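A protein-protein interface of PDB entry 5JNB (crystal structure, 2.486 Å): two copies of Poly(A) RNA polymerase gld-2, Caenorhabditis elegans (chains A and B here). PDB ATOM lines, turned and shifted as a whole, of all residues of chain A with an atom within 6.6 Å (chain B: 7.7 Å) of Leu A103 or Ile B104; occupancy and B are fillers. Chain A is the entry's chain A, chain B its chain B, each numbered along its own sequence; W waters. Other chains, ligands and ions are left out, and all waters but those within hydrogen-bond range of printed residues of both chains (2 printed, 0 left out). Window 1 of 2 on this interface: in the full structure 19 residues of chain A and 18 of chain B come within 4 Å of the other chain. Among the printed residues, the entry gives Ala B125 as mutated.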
ATOM      1  N   ALA A  81     -28.875 -11.680  22.304  1.00  0.00           N
ATOM      2  CA  ALA A  81     -27.780 -11.063  21.549  1.00  0.00           C
ATOM      3  C   ALA A  81     -27.828 -11.496  20.081  1.00  0.00           C
ATOM      4  O   ALA A  81     -27.348 -10.787  19.189  1.00  0.00           O
ATOM      5  CB  ALA A  81     -26.435 -11.398  22.165  1.00  0.00           C
ATOM      6  N   VAL A  82     -28.428 -12.648  19.831  1.00  0.00           N
ATOM      7  CA  VAL A  82     -28.556 -13.141  18.469  1.00  0.00           C
ATOM      8  C   VAL A  82     -29.563 -12.302  17.685  1.00  0.00           C
ATOM      9  O   VAL A  82     -29.290 -11.899  16.553  1.00  0.00           O
ATOM     10  CB  VAL A  82     -28.950 -14.634  18.473  1.00  0.00           C
ATOM     11  CG1 VAL A  82     -29.042 -15.162  17.091  1.00  0.00           C
ATOM     12  CG2 VAL A  82     -27.920 -15.419  19.266  1.00  0.00           C
ATOM     13  N   VAL A  83     -30.711 -12.010  18.297  1.00  0.00           N
ATOM     14  CA  VAL A  83     -31.663 -11.061  17.717  1.00  0.00           C
ATOM     15  C   VAL A  83     -31.003  -9.704  17.364  1.00  0.00           C
ATOM     16  O   VAL A  83     -31.103  -9.247  16.232  1.00  0.00           O
ATOM     17  CB  VAL A  83     -32.870 -10.831  18.677  1.00  0.00           C
ATOM     18  CG1 VAL A  83     -33.854  -9.823  18.088  1.00  0.00           C
ATOM     19  CG2 VAL A  83     -33.581 -12.160  18.962  1.00  0.00           C
ATOM     20  N   LEU A  85     -27.698  -8.902  16.974  1.00  0.00           N
ATOM     21  CA  LEU A  85     -26.717  -9.076  15.889  1.00  0.00           C
ATOM     22  C   LEU A  85     -27.373  -9.350  14.537  1.00  0.00           C
ATOM     23  O   LEU A  85     -26.862  -8.927  13.491  1.00  0.00           O
ATOM     24  CB  LEU A  85     -25.737 -10.201  16.215  1.00  0.00           C
ATOM     25  CG  LEU A  85     -24.878  -9.836  17.433  1.00  0.00           C
ATOM     26  CD1 LEU A  85     -23.926 -10.950  17.892  1.00  0.00           C
ATOM     27  CD2 LEU A  85     -24.144  -8.514  17.155  1.00  0.00           C
ATOM     28  N   ASN A  86     -28.503 -10.052  14.551  1.00  0.00           N
ATOM     29  CA  ASN A  86     -29.183 -10.376  13.299  1.00  0.00           C
ATOM     30  C   ASN A  86     -29.885  -9.147  12.778  1.00  0.00           C
ATOM     31  O   ASN A  86     -29.981  -8.949  11.560  1.00  0.00           O
ATOM     32  CB  ASN A  86     -30.184 -11.534  13.463  1.00  0.00           C
ATOM     33  CG  ASN A  86     -30.691 -12.058  12.117  1.00  0.00           C
ATOM     34  OD1 ASN A  86     -29.907 -12.323  11.193  1.00  0.00           O
ATOM     35  ND2 ASN A  86     -32.004 -12.190  11.994  1.00  0.00           N
ATOM     36  N   LEU A  89     -27.099  -7.115  11.252  1.00  0.00           N
ATOM     37  CA  LEU A  89     -26.776  -7.753   9.982  1.00  0.00           C
ATOM     38  C   LEU A  89     -27.725  -7.266   8.885  1.00  0.00           C
ATOM     39  O   LEU A  89     -27.265  -6.854   7.821  1.00  0.00           O
ATOM     40  CB  LEU A  89     -26.849  -9.274  10.127  1.00  0.00           C
ATOM     41  CG  LEU A  89     -26.429 -10.221   8.994  1.00  0.00           C
ATOM     42  CD1 LEU A  89     -26.054 -11.546   9.603  1.00  0.00           C
ATOM     43  CD2 LEU A  89     -27.534 -10.416   7.961  1.00  0.00           C
ATOM     44  N   GLN A 101     -21.151 -10.738   5.586  1.00  0.00           N
ATOM     45  CA  GLN A 101     -21.410 -10.875   7.008  1.00  0.00           C
ATOM     46  C   GLN A 101     -21.725 -12.323   7.383  1.00  0.00           C
ATOM     47  O   GLN A 101     -22.101 -13.127   6.525  1.00  0.00           O
ATOM     48  CB  GLN A 101     -22.566  -9.997   7.418  1.00  0.00           C
ATOM     49  CG  GLN A 101     -22.394  -8.565   7.039  1.00  0.00           C
ATOM     50  CD  GLN A 101     -23.493  -7.721   7.586  1.00  0.00           C
ATOM     51  OE1 GLN A 101     -23.351  -7.132   8.656  1.00  0.00           O
ATOM     52  NE2 GLN A 101     -24.615  -7.659   6.871  1.00  0.00           N
ATOM     53  N   LYS A 102     -21.611 -12.626   8.672  1.00  0.00           N
ATOM     54  CA  LYS A 102     -21.722 -13.979   9.177  1.00  0.00           C
ATOM     55  C   LYS A 102     -21.764 -14.019  10.705  1.00  0.00           C
ATOM     56  O   LYS A 102     -20.944 -13.397  11.365  1.00  0.00           O
ATOM     57  CB  LYS A 102     -20.538 -14.790   8.671  1.00  0.00           C
ATOM     58  CG  LYS A 102     -20.548 -16.232   9.022  1.00  0.00           C
ATOM     59  CD  LYS A 102     -19.155 -16.770   8.820  1.00  0.00           C
ATOM     60  CE  LYS A 102     -18.501 -16.162   7.582  1.00  0.00           C
ATOM     61  NZ  LYS A 102     -17.178 -16.781   7.293  1.00  0.00           N
ATOM     62  N   LEU A 103     -22.707 -14.772  11.259  1.00  0.00           N
ATOM     63  CA  LEU A 103     -22.832 -14.909  12.702  1.00  0.00           C
ATOM     64  C   LEU A 103     -22.090 -16.150  13.219  1.00  0.00           C
ATOM     65  O   LEU A 103     -22.443 -17.283  12.904  1.00  0.00           O
ATOM     66  CB  LEU A 103     -24.314 -14.950  13.108  1.00  0.00           C
ATOM     67  CG  LEU A 103     -24.770 -13.670  13.817  1.00  0.00           C
ATOM     68  CD1 LEU A 103     -26.262 -13.615  14.096  1.00  0.00           C
ATOM     69  CD2 LEU A 103     -24.007 -13.539  15.120  1.00  0.00           C
ATOM     70  N   ILE A 104     -21.068 -15.902  14.035  1.00  0.00           N
ATOM     71  CA  ILE A 104     -20.188 -16.925  14.582  1.00  0.00           C
ATOM     72  C   ILE A 104     -20.544 -17.175  16.026  1.00  0.00           C
ATOM     73  O   ILE A 104     -20.809 -16.230  16.759  1.00  0.00           O
ATOM     74  CB  ILE A 104     -18.705 -16.488  14.502  1.00  0.00           C
ATOM     75  CG1 ILE A 104     -18.253 -16.419  13.051  1.00  0.00           C
ATOM     76  CG2 ILE A 104     -17.798 -17.414  15.291  1.00  0.00           C
ATOM     77  CD1 ILE A 104     -18.727 -17.569  12.272  1.00  0.00           C
ATOM     78  N   LEU A 105     -20.573 -18.435  16.437  1.00  0.00           N
ATOM     79  CA  LEU A 105     -20.639 -18.735  17.854  1.00  0.00           C
ATOM     80  C   LEU A 105     -19.236 -18.829  18.437  1.00  0.00           C
ATOM     81  O   LEU A 105     -18.578 -19.849  18.269  1.00  0.00           O
ATOM     82  CB  LEU A 105     -21.402 -20.042  18.108  1.00  0.00           C
ATOM     83  CG  LEU A 105     -22.888 -19.989  17.734  1.00  0.00           C
ATOM     84  CD1 LEU A 105     -23.689 -21.137  18.345  1.00  0.00           C
ATOM     85  CD2 LEU A 105     -23.496 -18.645  18.158  1.00  0.00           C
ATOM     86  N   PRO A 109     -21.901 -14.809  20.996  1.00  0.00           N
ATOM     87  CA  PRO A 109     -22.128 -14.605  19.552  1.00  0.00           C
ATOM     88  C   PRO A 109     -21.375 -13.393  19.002  1.00  0.00           C
ATOM     89  O   PRO A 109     -21.228 -12.373  19.697  1.00  0.00           O
ATOM     90  CB  PRO A 109     -23.636 -14.382  19.456  1.00  0.00           C
ATOM     91  CG  PRO A 109     -24.193 -14.958  20.696  1.00  0.00           C
ATOM     92  CD  PRO A 109     -23.155 -14.728  21.758  1.00  0.00           C
ATOM     93  N   ILE A 110     -20.902 -13.513  17.766  1.00  0.00           N
ATOM     94  CA  ILE A 110     -19.996 -12.535  17.147  1.00  0.00           C
ATOM     95  C   ILE A 110     -20.375 -12.298  15.688  1.00  0.00           C
ATOM     96  O   ILE A 110     -20.412 -13.236  14.895  1.00  0.00           O
ATOM     97  CB  ILE A 110     -18.515 -13.015  17.193  1.00  0.00           C
ATOM     98  CG1 ILE A 110     -18.035 -13.144  18.633  1.00  0.00           C
ATOM     99  CG2 ILE A 110     -17.602 -12.079  16.411  1.00  0.00           C
ATOM    100  CD1 ILE A 110     -18.042 -11.841  19.370  1.00  0.00           C
ATOM    101  N   LEU A 111     -20.650 -11.052  15.327  1.00  0.00           N
ATOM    102  CA  LEU A 111     -20.949 -10.714  13.935  1.00  0.00           C
ATOM    103  C   LEU A 111     -19.649 -10.392  13.196  1.00  0.00           C
ATOM    104  O   LEU A 111     -18.981  -9.394  13.471  1.00  0.00           O
ATOM    105  CB  LEU A 111     -21.948  -9.546  13.859  1.00  0.00           C
ATOM    106  CG  LEU A 111     -22.402  -9.055  12.467  1.00  0.00           C
ATOM    107  CD1 LEU A 111     -23.050 -10.165  11.613  1.00  0.00           C
ATOM    108  CD2 LEU A 111     -23.349  -7.871  12.579  1.00  0.00           C
ATOM    109  N   ARG A 112     -19.292 -11.249  12.255  1.00  0.00           N
ATOM    110  CA  ARG A 112     -18.055 -11.081  11.512  1.00  0.00           C
ATOM    111  C   ARG A 112     -18.334 -10.375  10.180  1.00  0.00           C
ATOM    112  O   ARG A 112     -19.236 -10.779   9.439  1.00  0.00           O
ATOM    113  CB  ARG A 112     -17.395 -12.440  11.298  1.00  0.00           C
ATOM    114  CG  ARG A 112     -16.067 -12.408  10.566  1.00  0.00           C
ATOM    115  CD  ARG A 112     -15.674 -13.815  10.160  1.00  0.00           C
ATOM    116  NE  ARG A 112     -14.451 -13.856   9.369  1.00  0.00           N
ATOM    117  CZ  ARG A 112     -14.036 -14.932   8.707  1.00  0.00           C
ATOM    118  NH1 ARG A 112     -12.909 -14.888   8.003  1.00  0.00           N
ATOM    119  NH2 ARG A 112     -14.752 -16.052   8.754  1.00  0.00           N
ATOM    120  N   LEU A 126     -17.827  -8.029  15.876  1.00  0.00           N
ATOM    121  CA  LEU A 126     -18.724  -7.202  16.668  1.00  0.00           C
ATOM    122  C   LEU A 126     -19.507  -8.044  17.665  1.00  0.00           C
ATOM    123  O   LEU A 126     -20.182  -9.012  17.291  1.00  0.00           O
ATOM    124  CB  LEU A 126     -19.712  -6.441  15.768  1.00  0.00           C
ATOM    125  CG  LEU A 126     -20.735  -5.599  16.565  1.00  0.00           C
ATOM    126  CD1 LEU A 126     -20.068  -4.329  17.107  1.00  0.00           C
ATOM    127  CD2 LEU A 126     -21.986  -5.247  15.775  1.00  0.00           C
ATOM    128  N   VAL B  82     -26.391 -26.873  19.538  1.00  0.00           N
ATOM    129  CA  VAL B  82     -25.114 -26.192  19.747  1.00  0.00           C
ATOM    130  C   VAL B  82     -24.234 -26.993  20.704  1.00  0.00           C
ATOM    131  O   VAL B  82     -23.029 -27.149  20.492  1.00  0.00           O
ATOM    132  CB  VAL B  82     -25.338 -24.760  20.295  1.00  0.00           C
ATOM    133  CG1 VAL B  82     -24.036 -24.099  20.654  1.00  0.00           C
ATOM    134  CG2 VAL B  82     -26.097 -23.933  19.278  1.00  0.00           C
ATOM    135  N   LEU B  85     -23.060 -29.980  18.498  1.00  0.00           N
ATOM    136  CA  LEU B  85     -22.025 -29.579  17.545  1.00  0.00           C
ATOM    137  C   LEU B  85     -20.734 -29.208  18.259  1.00  0.00           C
ATOM    138  O   LEU B  85     -19.638 -29.452  17.748  1.00  0.00           O
ATOM    139  CB  LEU B  85     -22.507 -28.422  16.671  1.00  0.00           C
ATOM    140  CG  LEU B  85     -23.643 -28.837  15.715  1.00  0.00           C
ATOM    141  CD1 LEU B  85     -24.064 -27.727  14.763  1.00  0.00           C
ATOM    142  CD2 LEU B  85     -23.213 -30.077  14.940  1.00  0.00           C
ATOM    143  N   GLN B 101     -11.978 -25.596  12.465  1.00  0.00           N
ATOM    144  CA  GLN B 101     -13.420 -25.684  12.673  1.00  0.00           C
ATOM    145  C   GLN B 101     -13.991 -24.382  13.201  1.00  0.00           C
ATOM    146  O   GLN B 101     -13.289 -23.613  13.834  1.00  0.00           O
ATOM    147  CB  GLN B 101     -13.782 -26.766  13.667  1.00  0.00           C
ATOM    148  CG  GLN B 101     -13.658 -28.151  13.191  1.00  0.00           C
ATOM    149  CD  GLN B 101     -13.887 -29.110  14.322  1.00  0.00           C
ATOM    150  OE1 GLN B 101     -14.875 -29.858  14.340  1.00  0.00           O
ATOM    151  NE2 GLN B 101     -12.983 -29.082  15.294  1.00  0.00           N
ATOM    152  N   LYS B 102     -15.293 -24.205  12.988  1.00  0.00           N
ATOM    153  CA  LYS B 102     -16.013 -23.013  13.360  1.00  0.00           C
ATOM    154  C   LYS B 102     -17.524 -23.291  13.459  1.00  0.00           C
ATOM    155  O   LYS B 102     -18.092 -24.021  12.656  1.00  0.00           O
ATOM    156  CB  LYS B 102     -15.708 -21.913  12.339  1.00  0.00           C
ATOM    157  CG  LYS B 102     -16.594 -20.734  12.391  1.00  0.00           C
ATOM    158  CD  LYS B 102     -15.928 -19.568  11.698  1.00  0.00           C
ATOM    159  CE  LYS B 102     -15.137 -19.999  10.480  1.00  0.00           C
ATOM    160  NZ  LYS B 102     -14.722 -18.791   9.720  1.00  0.00           N
ATOM    161  N   LEU B 103     -18.162 -22.705  14.459  1.00  0.00           N
ATOM    162  CA  LEU B 103     -19.599 -22.794  14.640  1.00  0.00           C
ATOM    163  C   LEU B 103     -20.297 -21.553  14.091  1.00  0.00           C
ATOM    164  O   LEU B 103     -20.168 -20.489  14.672  1.00  0.00           O
ATOM    165  CB  LEU B 103     -19.929 -22.944  16.129  1.00  0.00           C
ATOM    166  CG  LEU B 103     -20.619 -24.228  16.558  1.00  0.00           C
ATOM    167  CD1 LEU B 103     -21.081 -24.104  17.987  1.00  0.00           C
ATOM    168  CD2 LEU B 103     -21.805 -24.523  15.630  1.00  0.00           C
ATOM    169  N   ILE B 104     -21.040 -21.658  12.994  1.00  0.00           N
ATOM    170  CA  ILE B 104     -21.782 -20.496  12.537  1.00  0.00           C
ATOM    171  C   ILE B 104     -23.270 -20.686  12.755  1.00  0.00           C
ATOM    172  O   ILE B 104     -23.738 -21.778  13.008  1.00  0.00           O
ATOM    173  CB  ILE B 104     -21.548 -20.184  11.067  1.00  0.00           C
ATOM    174  CG1 ILE B 104     -22.469 -21.064  10.210  1.00  0.00           C
ATOM    175  CG2 ILE B 104     -20.077 -20.353  10.739  1.00  0.00           C
ATOM    176  CD1 ILE B 104     -22.366 -20.856   8.720  1.00  0.00           C
ATOM    177  N   LEU B 105     -24.003 -19.591  12.680  1.00  0.00           N
ATOM    178  CA  LEU B 105     -25.446 -19.621  12.805  1.00  0.00           C
ATOM    179  C   LEU B 105     -26.067 -19.346  11.439  1.00  0.00           C
ATOM    180  O   LEU B 105     -26.035 -18.200  10.987  1.00  0.00           O
ATOM    181  CB  LEU B 105     -25.915 -18.579  13.813  1.00  0.00           C
ATOM    182  CG  LEU B 105     -26.865 -18.998  14.924  1.00  0.00           C
ATOM    183  CD1 LEU B 105     -26.250 -20.096  15.789  1.00  0.00           C
ATOM    184  CD2 LEU B 105     -27.198 -17.781  15.750  1.00  0.00           C
ATOM    185  N   ALA B 106     -26.590 -20.392  10.786  1.00  0.00           N
ATOM    186  CA  ALA B 106     -27.371 -20.247   9.567  1.00  0.00           C
ATOM    187  C   ALA B 106     -28.837 -20.353   9.963  1.00  0.00           C
ATOM    188  O   ALA B 106     -29.172 -19.967  11.065  1.00  0.00           O
ATOM    189  CB  ALA B 106     -26.986 -21.303   8.522  1.00  0.00           C
ATOM    190  N   LYS B 107     -29.719 -20.879   9.107  1.00  0.00           N
ATOM    191  CA  LYS B 107     -31.107 -21.060   9.545  1.00  0.00           C
ATOM    192  C   LYS B 107     -31.108 -22.052  10.700  1.00  0.00           C
ATOM    193  O   LYS B 107     -32.022 -22.093  11.516  1.00  0.00           O
ATOM    194  CB  LYS B 107     -32.021 -21.535   8.412  1.00  0.00           C
ATOM    195  CG  LYS B 107     -32.359 -20.478   7.368  1.00  0.00           C
ATOM    196  CD  LYS B 107     -33.388 -21.017   6.415  1.00  0.00           C
ATOM    197  CE  LYS B 107     -34.055 -19.944   5.561  1.00  0.00           C
ATOM    198  NZ  LYS B 107     -33.253 -19.465   4.392  1.00  0.00           N
ATOM    199  N   VAL B 108     -30.032 -22.804  10.812  1.00  0.00           N
ATOM    200  CA  VAL B 108     -29.886 -23.723  11.916  1.00  0.00           C
ATOM    201  C   VAL B 108     -28.380 -23.628  12.290  1.00  0.00           C
ATOM    202  O   VAL B 108     -27.590 -23.113  11.497  1.00  0.00           O
ATOM    203  CB  VAL B 108     -30.402 -25.126  11.427  1.00  0.00           C
ATOM    204  CG1 VAL B 108     -29.272 -26.066  10.950  1.00  0.00           C
ATOM    205  CG2 VAL B 108     -31.351 -25.746  12.380  1.00  0.00           C
ATOM    206  N   PRO B 109     -27.966 -24.070  13.492  1.00  0.00           N
ATOM    207  CA  PRO B 109     -26.526 -24.090  13.801  1.00  0.00           C
ATOM    208  C   PRO B 109     -25.781 -25.042  12.859  1.00  0.00           C
ATOM    209  O   PRO B 109     -26.335 -26.091  12.473  1.00  0.00           O
ATOM    210  CB  PRO B 109     -26.464 -24.613  15.233  1.00  0.00           C
ATOM    211  CG  PRO B 109     -27.826 -24.498  15.758  1.00  0.00           C
ATOM    212  CD  PRO B 109     -28.774 -24.569  14.611  1.00  0.00           C
ATOM    213  N   ILE B 110     -24.552 -24.684  12.492  1.00  0.00           N
ATOM    214  CA  ILE B 110     -23.800 -25.397  11.455  1.00  0.00           C
ATOM    215  C   ILE B 110     -22.320 -25.441  11.813  1.00  0.00           C
ATOM    216  O   ILE B 110     -21.704 -24.416  12.082  1.00  0.00           O
ATOM    217  CB  ILE B 110     -23.926 -24.731  10.057  1.00  0.00           C
ATOM    218  CG1 ILE B 110     -25.367 -24.750   9.523  1.00  0.00           C
ATOM    219  CG2 ILE B 110     -22.992 -25.410   9.074  1.00  0.00           C
ATOM    220  CD1 ILE B 110     -25.839 -26.128   9.061  1.00  0.00           C
ATOM    221  N   LEU B 111     -21.753 -26.636  11.808  1.00  0.00           N
ATOM    222  CA  LEU B 111     -20.345 -26.815  12.050  1.00  0.00           C
ATOM    223  C   LEU B 111     -19.578 -26.810  10.737  1.00  0.00           C
ATOM    224  O   LEU B 111     -19.775 -27.691   9.897  1.00  0.00           O
ATOM    225  CB  LEU B 111     -20.123 -28.118  12.808  1.00  0.00           C
ATOM    226  CG  LEU B 111     -18.710 -28.374  13.306  1.00  0.00           C
ATOM    227  CD1 LEU B 111     -18.295 -27.242  14.251  1.00  0.00           C
ATOM    228  CD2 LEU B 111     -18.641 -29.746  14.004  1.00  0.00           C
ATOM    229  N   ARG B 112     -18.729 -25.803  10.549  1.00  0.00           N
ATOM    230  CA  ARG B 112     -17.882 -25.714   9.362  1.00  0.00           C
ATOM    231  C   ARG B 112     -16.538 -26.316   9.642  1.00  0.00           C
ATOM    232  O   ARG B 112     -15.932 -26.013  10.671  1.00  0.00           O
ATOM    233  CB  ARG B 112     -17.683 -24.270   8.917  1.00  0.00           C
ATOM    234  CG  ARG B 112     -18.893 -23.606   8.353  1.00  0.00           C
ATOM    235  CD  ARG B 112     -18.497 -22.874   7.097  1.00  0.00           C
ATOM    236  NE  ARG B 112     -19.485 -23.093   6.053  1.00  0.00           N
ATOM    237  CZ  ARG B 112     -19.214 -23.036   4.756  1.00  0.00           C
ATOM    238  NH1 ARG B 112     -17.977 -22.765   4.344  1.00  0.00           N
ATOM    239  NH2 ARG B 112     -20.182 -23.247   3.873  1.00  0.00           N
ATOM    240  N   ALA B 125     -20.028 -28.767   5.852  1.00  0.00           N
ATOM    241  CA  ALA B 125     -21.062 -28.102   6.633  1.00  0.00           C
ATOM    242  C   ALA B 125     -21.942 -29.133   7.333  1.00  0.00           C
ATOM    243  O   ALA B 125     -22.761 -29.784   6.696  1.00  0.00           O
ATOM    244  CB  ALA B 125     -21.915 -27.203   5.739  1.00  0.00           C
ATOM    245  N   LEU B 126     -21.795 -29.262   8.644  1.00  0.00           N
ATOM    246  CA  LEU B 126     -22.494 -30.302   9.398  1.00  0.00           C
ATOM    247  C   LEU B 126     -23.616 -29.719  10.260  1.00  0.00           C
ATOM    248  O   LEU B 126     -23.349 -28.840  11.073  1.00  0.00           O
ATOM    249  CB  LEU B 126     -21.494 -31.044  10.297  1.00  0.00           C
ATOM    250  CG  LEU B 126     -22.093 -32.030  11.305  1.00  0.00           C
ATOM    251  CD1 LEU B 126     -22.500 -33.284  10.536  1.00  0.00           C
ATOM    252  CD2 LEU B 126     -21.146 -32.375  12.445  1.00  0.00           C
HETATM  253  O   HOH W   1     -17.048 -21.094  16.519  1.00  0.00           O
HETATM  254  O   HOH W   2     -24.366 -16.581   9.802  1.00  0.00           O
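Leu A103 touches Leu B105, and with the chains exchanged Leu A105 touches Leu B103. Ile A104 touches Lys B102, but with the chains exchanged Lys A102 does not touch Ile B104 (4.2 Å). Ile B104 touches its own counterpart, Ile A104. Arg A112 touches Lys B102, but with the chains exchanged Lys A102 does not touch Arg B112 (6.2 Å). Positions printed for both chains: 82, 85, 101, 102, 103, 104, 105, 109, 110, 111, 112 and 126.
Hydrophobic or aromatic side chains of chain B within 4 Å of the printed part of chain A: Val B82, Leu B103, Ile B104 and Leu B105. Among the printed residues, 11 pairs touch across the chains.
The backbone carbonyl oxygen of Leu A103 is in hydrogen-bond range of the backbone NH of Leu B105 (2.8 Å). The backbone carbonyl oxygen (O) of Leu B103 lies within hydrogen-bond range of the backbone NH (N) of Leu A105, at 2.7 Å. The side-chain amino group (NZ) of Lys B102 sits close to the guanidinium group (NH2) of Arg A112.
Water W2 lies within hydrogen-bond range of O of Leu B105 (2.6 Å) and N of Leu A103 (2.9 Å). Water W1 lies within hydrogen-bond range of the backbone carbonyl oxygen of Leu A105 and the backbone NH of Leu B103.
CG1 of Val A82 touches CD2 of Leu B105, 3.5 Å away. Lys A102 touches Lys B102. O of Leu A103 touches CA of Ile B104, at 3.3 Å. CD1 of Ile A104 touches CD of Lys B102, at 3.5 Å. O of Leu B103 touches CA of Ile A104 (3.6 Å). Ile A104 touches Ile B104. Leu A105 touches Val B82 (CD1 to CG1, 3.8 Å). Leu B105 touches Leu A105 (CD1 to CD1, 3.8 Å).
Of chain B, only Ile B104 (3.3 Å) and Leu B105 (2.8 Å) come within 4 Å of Leu A103. Ile B104 touches just these residues of chain A: Leu A103 and Ile A104. Of the printed residues of chain A, Val B82 touches Leu A105 (3.8 Å). Of the printed residues of chain A, Leu B103 touches Ile A104 and Leu A105. Printed residues of chain B within 4 Å of Leu A105: Val B82 (3.8 Å), Leu B103 (2.7 Å) and Leu B105 (3.8 Å). Asn A86 touches none of the printed residues of chain B. The nearest residue of chain B that does not touch Leu A103 is Leu B103 (4.3 Å). The nearest printed residue of chain A that does not touch Leu B103 is Leu A103 (4.3 Å).
The backbone carbonyl oxygen (O) of Lys A102 is in hydrogen-bond range of the backbone NH (N) of Arg A112. The backbone NH (N) of Ile A104 is in hydrogen-bond range of the backbone carbonyl oxygen (O) of Ile A110 (2.9 Å). The backbone carbonyl oxygen of Lys B102 is in hydrogen-bond range of the backbone NH of Arg B112 (2.8 Å). N of Ile B104 sits at hydrogen-bond distance from O of Ile B110 (3.0 Å).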
